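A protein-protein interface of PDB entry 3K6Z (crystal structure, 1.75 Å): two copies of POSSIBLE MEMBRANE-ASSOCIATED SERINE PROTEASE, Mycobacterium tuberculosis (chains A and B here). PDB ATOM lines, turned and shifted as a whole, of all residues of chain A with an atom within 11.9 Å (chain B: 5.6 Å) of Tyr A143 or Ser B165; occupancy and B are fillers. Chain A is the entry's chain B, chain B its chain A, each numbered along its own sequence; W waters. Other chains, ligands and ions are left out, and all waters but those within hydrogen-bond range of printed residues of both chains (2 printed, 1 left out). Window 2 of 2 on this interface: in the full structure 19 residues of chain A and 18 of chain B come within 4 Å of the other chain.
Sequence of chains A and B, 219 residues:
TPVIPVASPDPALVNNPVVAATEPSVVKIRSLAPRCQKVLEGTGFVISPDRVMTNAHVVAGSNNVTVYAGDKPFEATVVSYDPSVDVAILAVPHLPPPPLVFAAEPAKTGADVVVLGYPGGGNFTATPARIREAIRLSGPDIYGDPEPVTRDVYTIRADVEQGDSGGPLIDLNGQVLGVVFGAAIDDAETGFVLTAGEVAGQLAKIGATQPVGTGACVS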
ATOM      1  N   SER A  84      -7.324  17.613   7.870  1.00  0.00           N
ATOM      2  CA  SER A  84      -8.349  17.956   8.861  1.00  0.00           C
ATOM      3  C   SER A  84      -7.777  18.732  10.048  1.00  0.00           C
ATOM      4  O   SER A  84      -8.510  19.102  10.965  1.00  0.00           O
ATOM      5  CB  SER A  84      -9.060  16.702   9.366  1.00  0.00           C
ATOM      6  OG  SER A  84      -8.213  15.953  10.225  1.00  0.00           O
ATOM      7  N   GLY A 139     -18.285  26.926  12.889  1.00  0.00           N
ATOM      8  CA  GLY A 139     -18.735  27.280  11.560  1.00  0.00           C
ATOM      9  C   GLY A 139     -19.871  26.371  11.153  1.00  0.00           C
ATOM     10  O   GLY A 139     -20.277  25.493  11.915  1.00  0.00           O
ATOM     11  N   PRO A 140     -20.401  26.581   9.941  1.00  0.00           N
ATOM     12  CA  PRO A 140     -21.347  25.632   9.366  1.00  0.00           C
ATOM     13  C   PRO A 140     -20.630  24.315   9.071  1.00  0.00           C
ATOM     14  O   PRO A 140     -19.407  24.301   8.877  1.00  0.00           O
ATOM     15  CB  PRO A 140     -21.784  26.313   8.062  1.00  0.00           C
ATOM     16  CG  PRO A 140     -20.668  27.259   7.730  1.00  0.00           C
ATOM     17  CD  PRO A 140     -20.128  27.721   9.045  1.00  0.00           C
ATOM     18  N   ASP A 141     -21.376  23.213   9.071  1.00  0.00           N
ATOM     19  CA  ASP A 141     -20.821  21.946   8.649  1.00  0.00           C
ATOM     20  C   ASP A 141     -20.787  21.972   7.133  1.00  0.00           C
ATOM     21  O   ASP A 141     -21.806  21.727   6.488  1.00  0.00           O
ATOM     22  CB  ASP A 141     -21.668  20.777   9.170  1.00  0.00           C
ATOM     23  CG  ASP A 141     -21.231  19.420   8.610  1.00  0.00           C
ATOM     24  OD1 ASP A 141     -22.033  18.463   8.691  1.00  0.00           O
ATOM     25  OD2 ASP A 141     -20.105  19.294   8.095  1.00  0.00           O
ATOM     26  N   ILE A 142     -19.628  22.300   6.567  1.00  0.00           N
ATOM     27  CA  ILE A 142     -19.463  22.266   5.113  1.00  0.00           C
ATOM     28  C   ILE A 142     -19.143  20.829   4.745  1.00  0.00           C
ATOM     29  O   ILE A 142     -18.087  20.308   5.094  1.00  0.00           O
ATOM     30  CB  ILE A 142     -18.348  23.229   4.606  1.00  0.00           C
ATOM     31  CG1 ILE A 142     -18.520  24.645   5.178  1.00  0.00           C
ATOM     32  CG2 ILE A 142     -18.254  23.212   3.071  1.00  0.00           C
ATOM     33  CD1 ILE A 142     -19.851  25.309   4.924  1.00  0.00           C
ATOM     34  N   TYR A 143     -20.075  20.190   4.046  1.00  0.00           N
ATOM     35  CA  TYR A 143     -19.983  18.772   3.735  1.00  0.00           C
ATOM     36  C   TYR A 143     -18.697  18.407   2.990  1.00  0.00           C
ATOM     37  O   TYR A 143     -18.420  18.932   1.909  1.00  0.00           O
ATOM     38  CB  TYR A 143     -21.194  18.342   2.907  1.00  0.00           C
ATOM     39  CG  TYR A 143     -22.518  18.315   3.643  1.00  0.00           C
ATOM     40  CD1 TYR A 143     -23.705  18.585   2.966  1.00  0.00           C
ATOM     41  CD2 TYR A 143     -22.594  18.009   5.008  1.00  0.00           C
ATOM     42  CE1 TYR A 143     -24.927  18.546   3.609  1.00  0.00           C
ATOM     43  CE2 TYR A 143     -23.835  17.965   5.666  1.00  0.00           C
ATOM     44  CZ  TYR A 143     -24.992  18.241   4.957  1.00  0.00           C
ATOM     45  OH  TYR A 143     -26.228  18.205   5.568  1.00  0.00           O
ATOM     46  N   GLY A 144     -17.916  17.508   3.587  1.00  0.00           N
ATOM     47  CA  GLY A 144     -16.678  17.023   2.976  1.00  0.00           C
ATOM     48  C   GLY A 144     -15.472  17.929   3.147  1.00  0.00           C
ATOM     49  O   GLY A 144     -14.359  17.572   2.741  1.00  0.00           O
ATOM     50  N   ASP A 145     -15.686  19.104   3.735  1.00  0.00           N
ATOM     51  CA  ASP A 145     -14.613  20.066   3.979  1.00  0.00           C
ATOM     52  C   ASP A 145     -13.718  19.546   5.103  1.00  0.00           C
ATOM     53  O   ASP A 145     -14.213  19.228   6.188  1.00  0.00           O
ATOM     54  CB  ASP A 145     -15.203  21.423   4.365  1.00  0.00           C
ATOM     55  CG  ASP A 145     -14.189  22.557   4.328  1.00  0.00           C
ATOM     56  OD1 ASP A 145     -12.967  22.313   4.405  1.00  0.00           O
ATOM     57  OD2 ASP A 145     -14.633  23.719   4.245  1.00  0.00           O
ATOM     58  N   PRO A 146     -12.403  19.428   4.830  1.00  0.00           N
ATOM     59  CA  PRO A 146     -11.406  18.986   5.811  1.00  0.00           C
ATOM     60  C   PRO A 146     -11.412  19.753   7.137  1.00  0.00           C
ATOM     61  O   PRO A 146     -11.483  19.120   8.198  1.00  0.00           O
ATOM     62  CB  PRO A 146     -10.069  19.176   5.073  1.00  0.00           C
ATOM     63  CG  PRO A 146     -10.372  20.018   3.889  1.00  0.00           C
ATOM     64  CD  PRO A 146     -11.777  19.687   3.520  1.00  0.00           C
ATOM     65  N   GLU A 147     -11.349  21.086   7.070  1.00  0.00           N
ATOM     66  CA  GLU A 147     -11.258  21.961   8.252  1.00  0.00           C
ATOM     67  C   GLU A 147     -12.135  21.479   9.415  1.00  0.00           C
ATOM     68  O   GLU A 147     -13.242  20.992   9.191  1.00  0.00           O
ATOM     69  CB  GLU A 147     -11.656  23.399   7.886  1.00  0.00           C
ATOM     70  CG  GLU A 147     -10.917  24.020   6.691  1.00  0.00           C
ATOM     71  CD  GLU A 147      -9.545  24.599   7.042  1.00  0.00           C
ATOM     72  OE1 GLU A 147      -8.606  24.426   6.236  1.00  0.00           O
ATOM     73  OE2 GLU A 147      -9.398  25.234   8.109  1.00  0.00           O
ATOM     74  N   PRO A 148     -11.641  21.593  10.666  1.00  0.00           N
ATOM     75  CA  PRO A 148     -12.545  21.285  11.783  1.00  0.00           C
ATOM     76  C   PRO A 148     -13.761  22.216  11.800  1.00  0.00           C
ATOM     77  O   PRO A 148     -13.636  23.392  11.454  1.00  0.00           O
ATOM     78  CB  PRO A 148     -11.681  21.518  13.032  1.00  0.00           C
ATOM     79  CG  PRO A 148     -10.479  22.273  12.571  1.00  0.00           C
ATOM     80  CD  PRO A 148     -10.286  21.962  11.119  1.00  0.00           C
ATOM     81  N   VAL A 149     -14.921  21.690  12.186  1.00  0.00           N
ATOM     82  CA  VAL A 149     -16.138  22.509  12.311  1.00  0.00           C
ATOM     83  C   VAL A 149     -16.069  23.442  13.530  1.00  0.00           C
ATOM     84  O   VAL A 149     -16.568  24.572  13.497  1.00  0.00           O
ATOM     85  CB  VAL A 149     -17.432  21.641  12.361  1.00  0.00           C
ATOM     86  CG1 VAL A 149     -17.393  20.636  13.520  1.00  0.00           C
ATOM     87  CG2 VAL A 149     -18.666  22.521  12.471  1.00  0.00           C
ATOM     88  N   THR A 150     -15.427  22.960  14.590  1.00  0.00           N
ATOM     89  CA  THR A 150     -15.384  23.665  15.861  1.00  0.00           C
ATOM     90  C   THR A 150     -13.942  23.674  16.368  1.00  0.00           C
ATOM     91  O   THR A 150     -13.228  22.676  16.242  1.00  0.00           O
ATOM     92  CB  THR A 150     -16.336  22.990  16.886  1.00  0.00           C
ATOM     93  OG1 THR A 150     -17.699  23.157  16.456  1.00  0.00           O
ATOM     94  CG2 THR A 150     -16.191  23.595  18.260  1.00  0.00           C
ATOM     95  N   GLU B  41     -18.559   9.931  -0.748  1.00  0.00           N
ATOM     96  CA  GLU B  41     -19.831   9.777  -1.445  1.00  0.00           C
ATOM     97  C   GLU B  41     -20.656  11.039  -1.339  1.00  0.00           C
ATOM     98  O   GLU B  41     -20.625  11.732  -0.320  1.00  0.00           O
ATOM     99  CB  GLU B  41     -20.612   8.594  -0.884  1.00  0.00           C
ATOM    100  CG  GLU B  41     -19.788   7.324  -0.768  1.00  0.00           C
ATOM    101  N   GLY B  42     -21.411  11.326  -2.392  1.00  0.00           N
ATOM    102  CA  GLY B  42     -22.184  12.548  -2.456  1.00  0.00           C
ATOM    103  C   GLY B  42     -23.207  12.431  -3.572  1.00  0.00           C
ATOM    104  O   GLY B  42     -23.556  11.330  -3.994  1.00  0.00           O
ATOM    105  N   THR B  43     -23.659  13.578  -4.051  1.00  0.00           N
ATOM    106  CA  THR B  43     -24.657  13.642  -5.122  1.00  0.00           C
ATOM    107  C   THR B  43     -24.145  14.580  -6.214  1.00  0.00           C
ATOM    108  O   THR B  43     -23.311  15.451  -5.958  1.00  0.00           O
ATOM    109  CB  THR B  43     -26.006  14.147  -4.552  1.00  0.00           C
ATOM    110  OG1 THR B  43     -26.463  13.231  -3.546  1.00  0.00           O
ATOM    111  CG2 THR B  43     -27.069  14.276  -5.640  1.00  0.00           C
ATOM    112  N   GLY B  44     -24.628  14.397  -7.438  1.00  0.00           N
ATOM    113  CA  GLY B  44     -24.358  15.349  -8.502  1.00  0.00           C
ATOM    114  C   GLY B  44     -25.572  15.453  -9.399  1.00  0.00           C
ATOM    115  O   GLY B  44     -26.571  14.757  -9.182  1.00  0.00           O
ATOM    116  N   THR B  54     -21.020  18.743  -9.125  1.00  0.00           N
ATOM    117  CA  THR B  54     -21.049  18.167  -7.790  1.00  0.00           C
ATOM    118  C   THR B  54     -20.262  19.038  -6.813  1.00  0.00           C
ATOM    119  O   THR B  54     -19.813  20.118  -7.175  1.00  0.00           O
ATOM    120  CB  THR B  54     -20.534  16.695  -7.791  1.00  0.00           C
ATOM    121  OG1 THR B  54     -20.731  16.113  -6.489  1.00  0.00           O
ATOM    122  CG2 THR B  54     -19.041  16.611  -8.199  1.00  0.00           C
ATOM    123  N   ASN B  55     -20.146  18.556  -5.580  1.00  0.00           N
ATOM    124  CA  ASN B  55     -19.368  19.182  -4.504  1.00  0.00           C
ATOM    125  C   ASN B  55     -17.879  18.913  -4.739  1.00  0.00           C
ATOM    126  O   ASN B  55     -17.468  17.764  -4.885  1.00  0.00           O
ATOM    127  CB  ASN B  55     -19.840  18.587  -3.159  1.00  0.00           C
ATOM    128  CG  ASN B  55     -18.977  19.003  -1.968  1.00  0.00           C
ATOM    129  OD1 ASN B  55     -18.329  20.051  -1.985  1.00  0.00           O
ATOM    130  ND2 ASN B  55     -18.987  18.174  -0.908  1.00  0.00           N
ATOM    131  N   HIS B  57     -15.572  18.914  -2.663  1.00  0.00           N
ATOM    132  CA  HIS B  57     -15.027  18.127  -1.548  1.00  0.00           C
ATOM    133  C   HIS B  57     -15.268  16.626  -1.639  1.00  0.00           C
ATOM    134  O   HIS B  57     -14.548  15.836  -1.015  1.00  0.00           O
ATOM    135  CB  HIS B  57     -15.541  18.680  -0.227  1.00  0.00           C
ATOM    136  CG  HIS B  57     -15.139  20.096   0.011  1.00  0.00           C
ATOM    137  ND1 HIS B  57     -13.838  20.457   0.294  1.00  0.00           N
ATOM    138  CD2 HIS B  57     -15.850  21.246  -0.026  1.00  0.00           C
ATOM    139  CE1 HIS B  57     -13.770  21.768   0.438  1.00  0.00           C
ATOM    140  NE2 HIS B  57     -14.976  22.270   0.253  1.00  0.00           N
ATOM    141  N   VAL B  58     -16.267  16.225  -2.418  1.00  0.00           N
ATOM    142  CA  VAL B  58     -16.513  14.804  -2.653  1.00  0.00           C
ATOM    143  C   VAL B  58     -15.394  14.225  -3.521  1.00  0.00           C
ATOM    144  O   VAL B  58     -14.938  13.101  -3.301  1.00  0.00           O
ATOM    145  CB  VAL B  58     -17.887  14.568  -3.323  1.00  0.00           C
ATOM    146  CG1 VAL B  58     -18.117  13.082  -3.603  1.00  0.00           C
ATOM    147  CG2 VAL B  58     -19.000  15.100  -2.449  1.00  0.00           C
ATOM    148  N   VAL B 160     -31.503  17.711   5.773  1.00  0.00           N
ATOM    149  CA  VAL B 160     -30.336  17.416   4.934  1.00  0.00           C
ATOM    150  C   VAL B 160     -29.383  16.412   5.586  1.00  0.00           C
ATOM    151  O   VAL B 160     -29.417  16.199   6.798  1.00  0.00           O
ATOM    152  CB  VAL B 160     -29.555  18.699   4.484  1.00  0.00           C
ATOM    153  CG1 VAL B 160     -30.259  19.371   3.303  1.00  0.00           C
ATOM    154  CG2 VAL B 160     -29.357  19.666   5.640  1.00  0.00           C
ATOM    155  N   GLU B 161     -28.544  15.796   4.761  1.00  0.00           N
ATOM    156  CA  GLU B 161     -27.558  14.823   5.208  1.00  0.00           C
ATOM    157  C   GLU B 161     -26.355  14.938   4.270  1.00  0.00           C
ATOM    158  O   GLU B 161     -26.513  15.326   3.108  1.00  0.00           O
ATOM    159  CB  GLU B 161     -28.167  13.421   5.182  1.00  0.00           C
ATOM    160  CG  GLU B 161     -27.491  12.409   6.082  1.00  0.00           C
ATOM    161  CD  GLU B 161     -26.364  11.652   5.397  1.00  0.00           C
ATOM    162  OE1 GLU B 161     -26.410  11.466   4.164  1.00  0.00           O
ATOM    163  OE2 GLU B 161     -25.433  11.226   6.103  1.00  0.00           O
ATOM    164  N   GLN B 162     -25.157  14.622   4.760  1.00  0.00           N
ATOM    165  CA  GLN B 162     -23.934  14.835   3.963  1.00  0.00           C
ATOM    166  C   GLN B 162     -23.965  14.185   2.579  1.00  0.00           C
ATOM    167  O   GLN B 162     -23.347  14.690   1.649  1.00  0.00           O
ATOM    168  CB  GLN B 162     -22.668  14.430   4.734  1.00  0.00           C
ATOM    169  CG  GLN B 162     -22.633  12.992   5.222  1.00  0.00           C
ATOM    170  CD  GLN B 162     -21.379  12.676   6.033  1.00  0.00           C
ATOM    171  OE1 GLN B 162     -21.301  11.639   6.688  1.00  0.00           O
ATOM    172  NE2 GLN B 162     -20.396  13.578   5.996  1.00  0.00           N
ATOM    173  N   GLY B 163     -24.691  13.076   2.449  1.00  0.00           N
ATOM    174  CA  GLY B 163     -24.879  12.421   1.149  1.00  0.00           C
ATOM    175  C   GLY B 163     -25.540  13.294   0.090  1.00  0.00           C
ATOM    176  O   GLY B 163     -25.360  13.062  -1.108  1.00  0.00           O
ATOM    177  N   ASP B 164     -26.319  14.285   0.527  1.00  0.00           N
ATOM    178  CA  ASP B 164     -26.986  15.226  -0.378  1.00  0.00           C
ATOM    179  C   ASP B 164     -26.003  16.221  -1.003  1.00  0.00           C
ATOM    180  O   ASP B 164     -26.339  16.899  -1.971  1.00  0.00           O
ATOM    181  CB  ASP B 164     -28.059  16.035   0.366  1.00  0.00           C
ATOM    182  CG  ASP B 164     -29.250  15.197   0.804  1.00  0.00           C
ATOM    183  OD1 ASP B 164     -29.673  14.296   0.050  1.00  0.00           O
ATOM    184  OD2 ASP B 164     -29.787  15.464   1.908  1.00  0.00           O
ATOM    185  N   SER B 165     -24.802  16.328  -0.435  1.00  0.00           N
ATOM    186  CA  SER B 165     -23.854  17.348  -0.894  1.00  0.00           C
ATOM    187  C   SER B 165     -23.586  17.206  -2.388  1.00  0.00           C
ATOM    188  O   SER B 165     -23.432  16.091  -2.890  1.00  0.00           O
ATOM    189  CB  SER B 165     -22.543  17.283  -0.109  1.00  0.00           C
ATOM    190  OG  SER B 165     -21.627  16.405  -0.735  1.00  0.00           O
ATOM    191  N   GLY B 166     -23.547  18.337  -3.092  1.00  0.00           N
ATOM    192  CA  GLY B 166     -23.426  18.344  -4.561  1.00  0.00           C
ATOM    193  C   GLY B 166     -24.754  18.214  -5.305  1.00  0.00           C
ATOM    194  O   GLY B 166     -24.813  18.435  -6.513  1.00  0.00           O
ATOM    195  N   GLY B 167     -25.807  17.837  -4.586  1.00  0.00           N
ATOM    196  CA  GLY B 167     -27.153  17.697  -5.169  1.00  0.00           C
ATOM    197  C   GLY B 167     -27.845  19.033  -5.434  1.00  0.00           C
ATOM    198  O   GLY B 167     -27.539  20.040  -4.782  1.00  0.00           O
ATOM    199  N   VAL B 180     -26.547  21.962  -2.982  1.00  0.00           N
ATOM    200  CA  VAL B 180     -26.489  21.672  -1.541  1.00  0.00           C
ATOM    201  C   VAL B 180     -25.029  21.549  -1.077  1.00  0.00           C
ATOM    202  O   VAL B 180     -24.250  20.796  -1.660  1.00  0.00           O
ATOM    203  CB  VAL B 180     -27.287  20.401  -1.185  1.00  0.00           C
ATOM    204  CG1 VAL B 180     -27.094  20.028   0.281  1.00  0.00           C
ATOM    205  CG2 VAL B 180     -28.775  20.615  -1.499  1.00  0.00           C
ATOM    206  N   PHE B 181     -24.648  22.286  -0.039  1.00  0.00           N
ATOM    207  CA  PHE B 181     -23.233  22.234   0.348  1.00  0.00           C
ATOM    208  C   PHE B 181     -22.926  22.130   1.851  1.00  0.00           C
ATOM    209  O   PHE B 181     -21.781  21.882   2.234  1.00  0.00           O
ATOM    210  CB  PHE B 181     -22.404  23.294  -0.427  1.00  0.00           C
ATOM    211  CG  PHE B 181     -21.981  24.493   0.393  1.00  0.00           C
ATOM    212  CD1 PHE B 181     -22.917  25.411   0.856  1.00  0.00           C
ATOM    213  CD2 PHE B 181     -20.635  24.708   0.667  1.00  0.00           C
ATOM    214  CE1 PHE B 181     -22.516  26.518   1.620  1.00  0.00           C
ATOM    215  CE2 PHE B 181     -20.221  25.805   1.419  1.00  0.00           C
ATOM    216  CZ  PHE B 181     -21.172  26.711   1.896  1.00  0.00           C
ATOM    217  N   GLY B 182     -23.946  22.265   2.697  1.00  0.00           N
ATOM    218  CA  GLY B 182     -23.741  22.090   4.137  1.00  0.00           C
ATOM    219  C   GLY B 182     -24.974  22.141   5.010  1.00  0.00           C
ATOM    220  O   GLY B 182     -26.102  22.224   4.519  1.00  0.00           O
ATOM    221  N   ALA B 183     -24.746  22.094   6.321  1.00  0.00           N
ATOM    222  CA  ALA B 183     -25.815  22.154   7.312  1.00  0.00           C
ATOM    223  C   ALA B 183     -25.366  22.966   8.527  1.00  0.00           C
ATOM    224  O   ALA B 183     -24.166  23.090   8.786  1.00  0.00           O
ATOM    225  CB  ALA B 183     -26.218  20.750   7.742  1.00  0.00           C
HETATM  226  O   HOH W   1     -21.339  15.709   7.933  1.00  0.00           O
HETATM  227  O   HOH W   2     -19.068  14.465   3.950  1.00  0.00           O
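Ala B183 touches Pro A140 (O to C, 3.8 Å).
Asp A141 touches Gly B182.
Tyr A143 touches His B57.
OH of Tyr A143 touches CG2 of Val B160, 3.5 Å away.
Gln B162 touches Tyr A143.
Tyr A143 touches Ser B165.
CD1 of Tyr A143 touches CA of Gly B182, at 3.7 Å.
Tyr A143 touches Ala B183.
CB of His B57 touches O of Gly A144, 3.4 Å away.
His B57 touches Pro A146 (ND1 to CD, 3.9 Å).
Hydrophobic or aromatic side chains of chain B within 4 Å of the printed part of chain A: His B57, Val B160, Phe B181 and Ala B183.
Printed residues of chain A that touch a printed residue of chain B: Pro A140, Asp A141, Ile A142, Tyr A143, Gly A144, Asp A145 and Pro A146.
Among the printed residues, 16 pairs touch across the chains.
Among the printed residues, no Asp or Glu carboxylate lies within 4 Å of a Lys or Arg side-chain nitrogen of the other chain.
The side-chain amide nitrogen (ND2) of Asn B55 lies within hydrogen-bond range of the side-chain hydroxyl (OG) of Ser B165 (3.2 Å).
The backbone carbonyl oxygen (O) of Gln B162 lies close to the side-chain hydroxyl (OG) of Ser B165 (3.4 Å).
N of Glu B161 is in hydrogen-bond range of OD2 of Asp B164, 3.1 Å away.
N of His B57 lies within hydrogen-bond range of OD1 of Asn B55.
The backbone NH of Gly B163 lies within hydrogen-bond range of the side-chain carboxylate of Glu B161 (2.9 Å).
The backbone NH of Thr B43 sits at hydrogen-bond distance from the backbone carbonyl oxygen of Ser B165.
Water W2 bridges the side-chain amide nitrogen (NE2) of Gln B162 (2.6 Å) and the backbone NH (N) of Gly A144 (3.3 Å).
Water W1 bridges OD1 of Asp A141 (2.9 Å) and NE2 of Gln B162 (3.0 Å).
No position is printed for both chains.
Of the 16 pairs that touch across the chains among the printed residues, none has its exchanged pair printed and touching as well.
Printed residues of chain B within 4 Å of Tyr A143: Asn B55 (3.0 Å), His B57 (3.6 Å), Val B160 (3.5 Å), Glu B161 (3.4 Å), Gln B162 (3.6 Å), Ser B165 (3.5 Å), Phe B181 (3.0 Å), Gly B182 (3.7 Å) and Ala B183 (3.3 Å).
No residue of chain A comes within 4 Å of Gly B42.
No residue of chain A comes within 4 Å of Thr B43.
No residue of chain A comes within 4 Å of Gly B44.
Thr B54 touches none of the printed residues of chain A.
Of chain A, only Tyr A143 comes within 4 Å of Asn B55.
Of chain A, only Tyr A143, Gly A144, Asp A145 and Pro A146 come within 4 Å of His B57.
Glu B161 touches one residue of chain A.
Gln B162 touches just one residue of chain A: Tyr A143 (3.6 Å).
No residue of chain A comes within 4 Å of Gly B163.
No residue of chain A comes within 4 Å of Gly B166.
No residue of chain A comes within 4 Å of Gly B167.
No residue of chain A comes within 4 Å of Val B180.
Phe B181 touches two residues of chain A.
Of the printed residues of chain A, Gly B182 touches Asp A141 and Tyr A143.
Printed residues of chain A within 4 Å of Ala B183: Pro A140 (3.8 Å), Asp A141 (2.8 Å) and Tyr A143 (3.3 Å).
Printed residues of chain B within 4 Å of Pro A140: Ala B183 (3.8 Å).
Printed residues of chain B within 4 Å of Pro A146: His B57 (3.9 Å).
The nearest residue of chain B that does not touch Tyr A143 is Val B180 (4.2 Å).
The nearest printed residue of chain B that does not touch Pro A140 is Phe B181 (5.9 Å).
The backbone NH of Glu B161 sits at hydrogen-bond distance from the side-chain hydroxyl of Tyr A143 (3.4 Å).
The backbone carbonyl oxygen of Ala B183 sits at hydrogen-bond distance from the backbone NH of Asp A141 (2.8 Å).
The side-chain amide nitrogen (ND2) of Asn B55 lies within hydrogen-bond range of the backbone carbonyl oxygen (O) of Tyr A143 (3.0 Å).
N of Tyr A143 lies within hydrogen-bond range of O of Phe B181 (3.0 Å).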
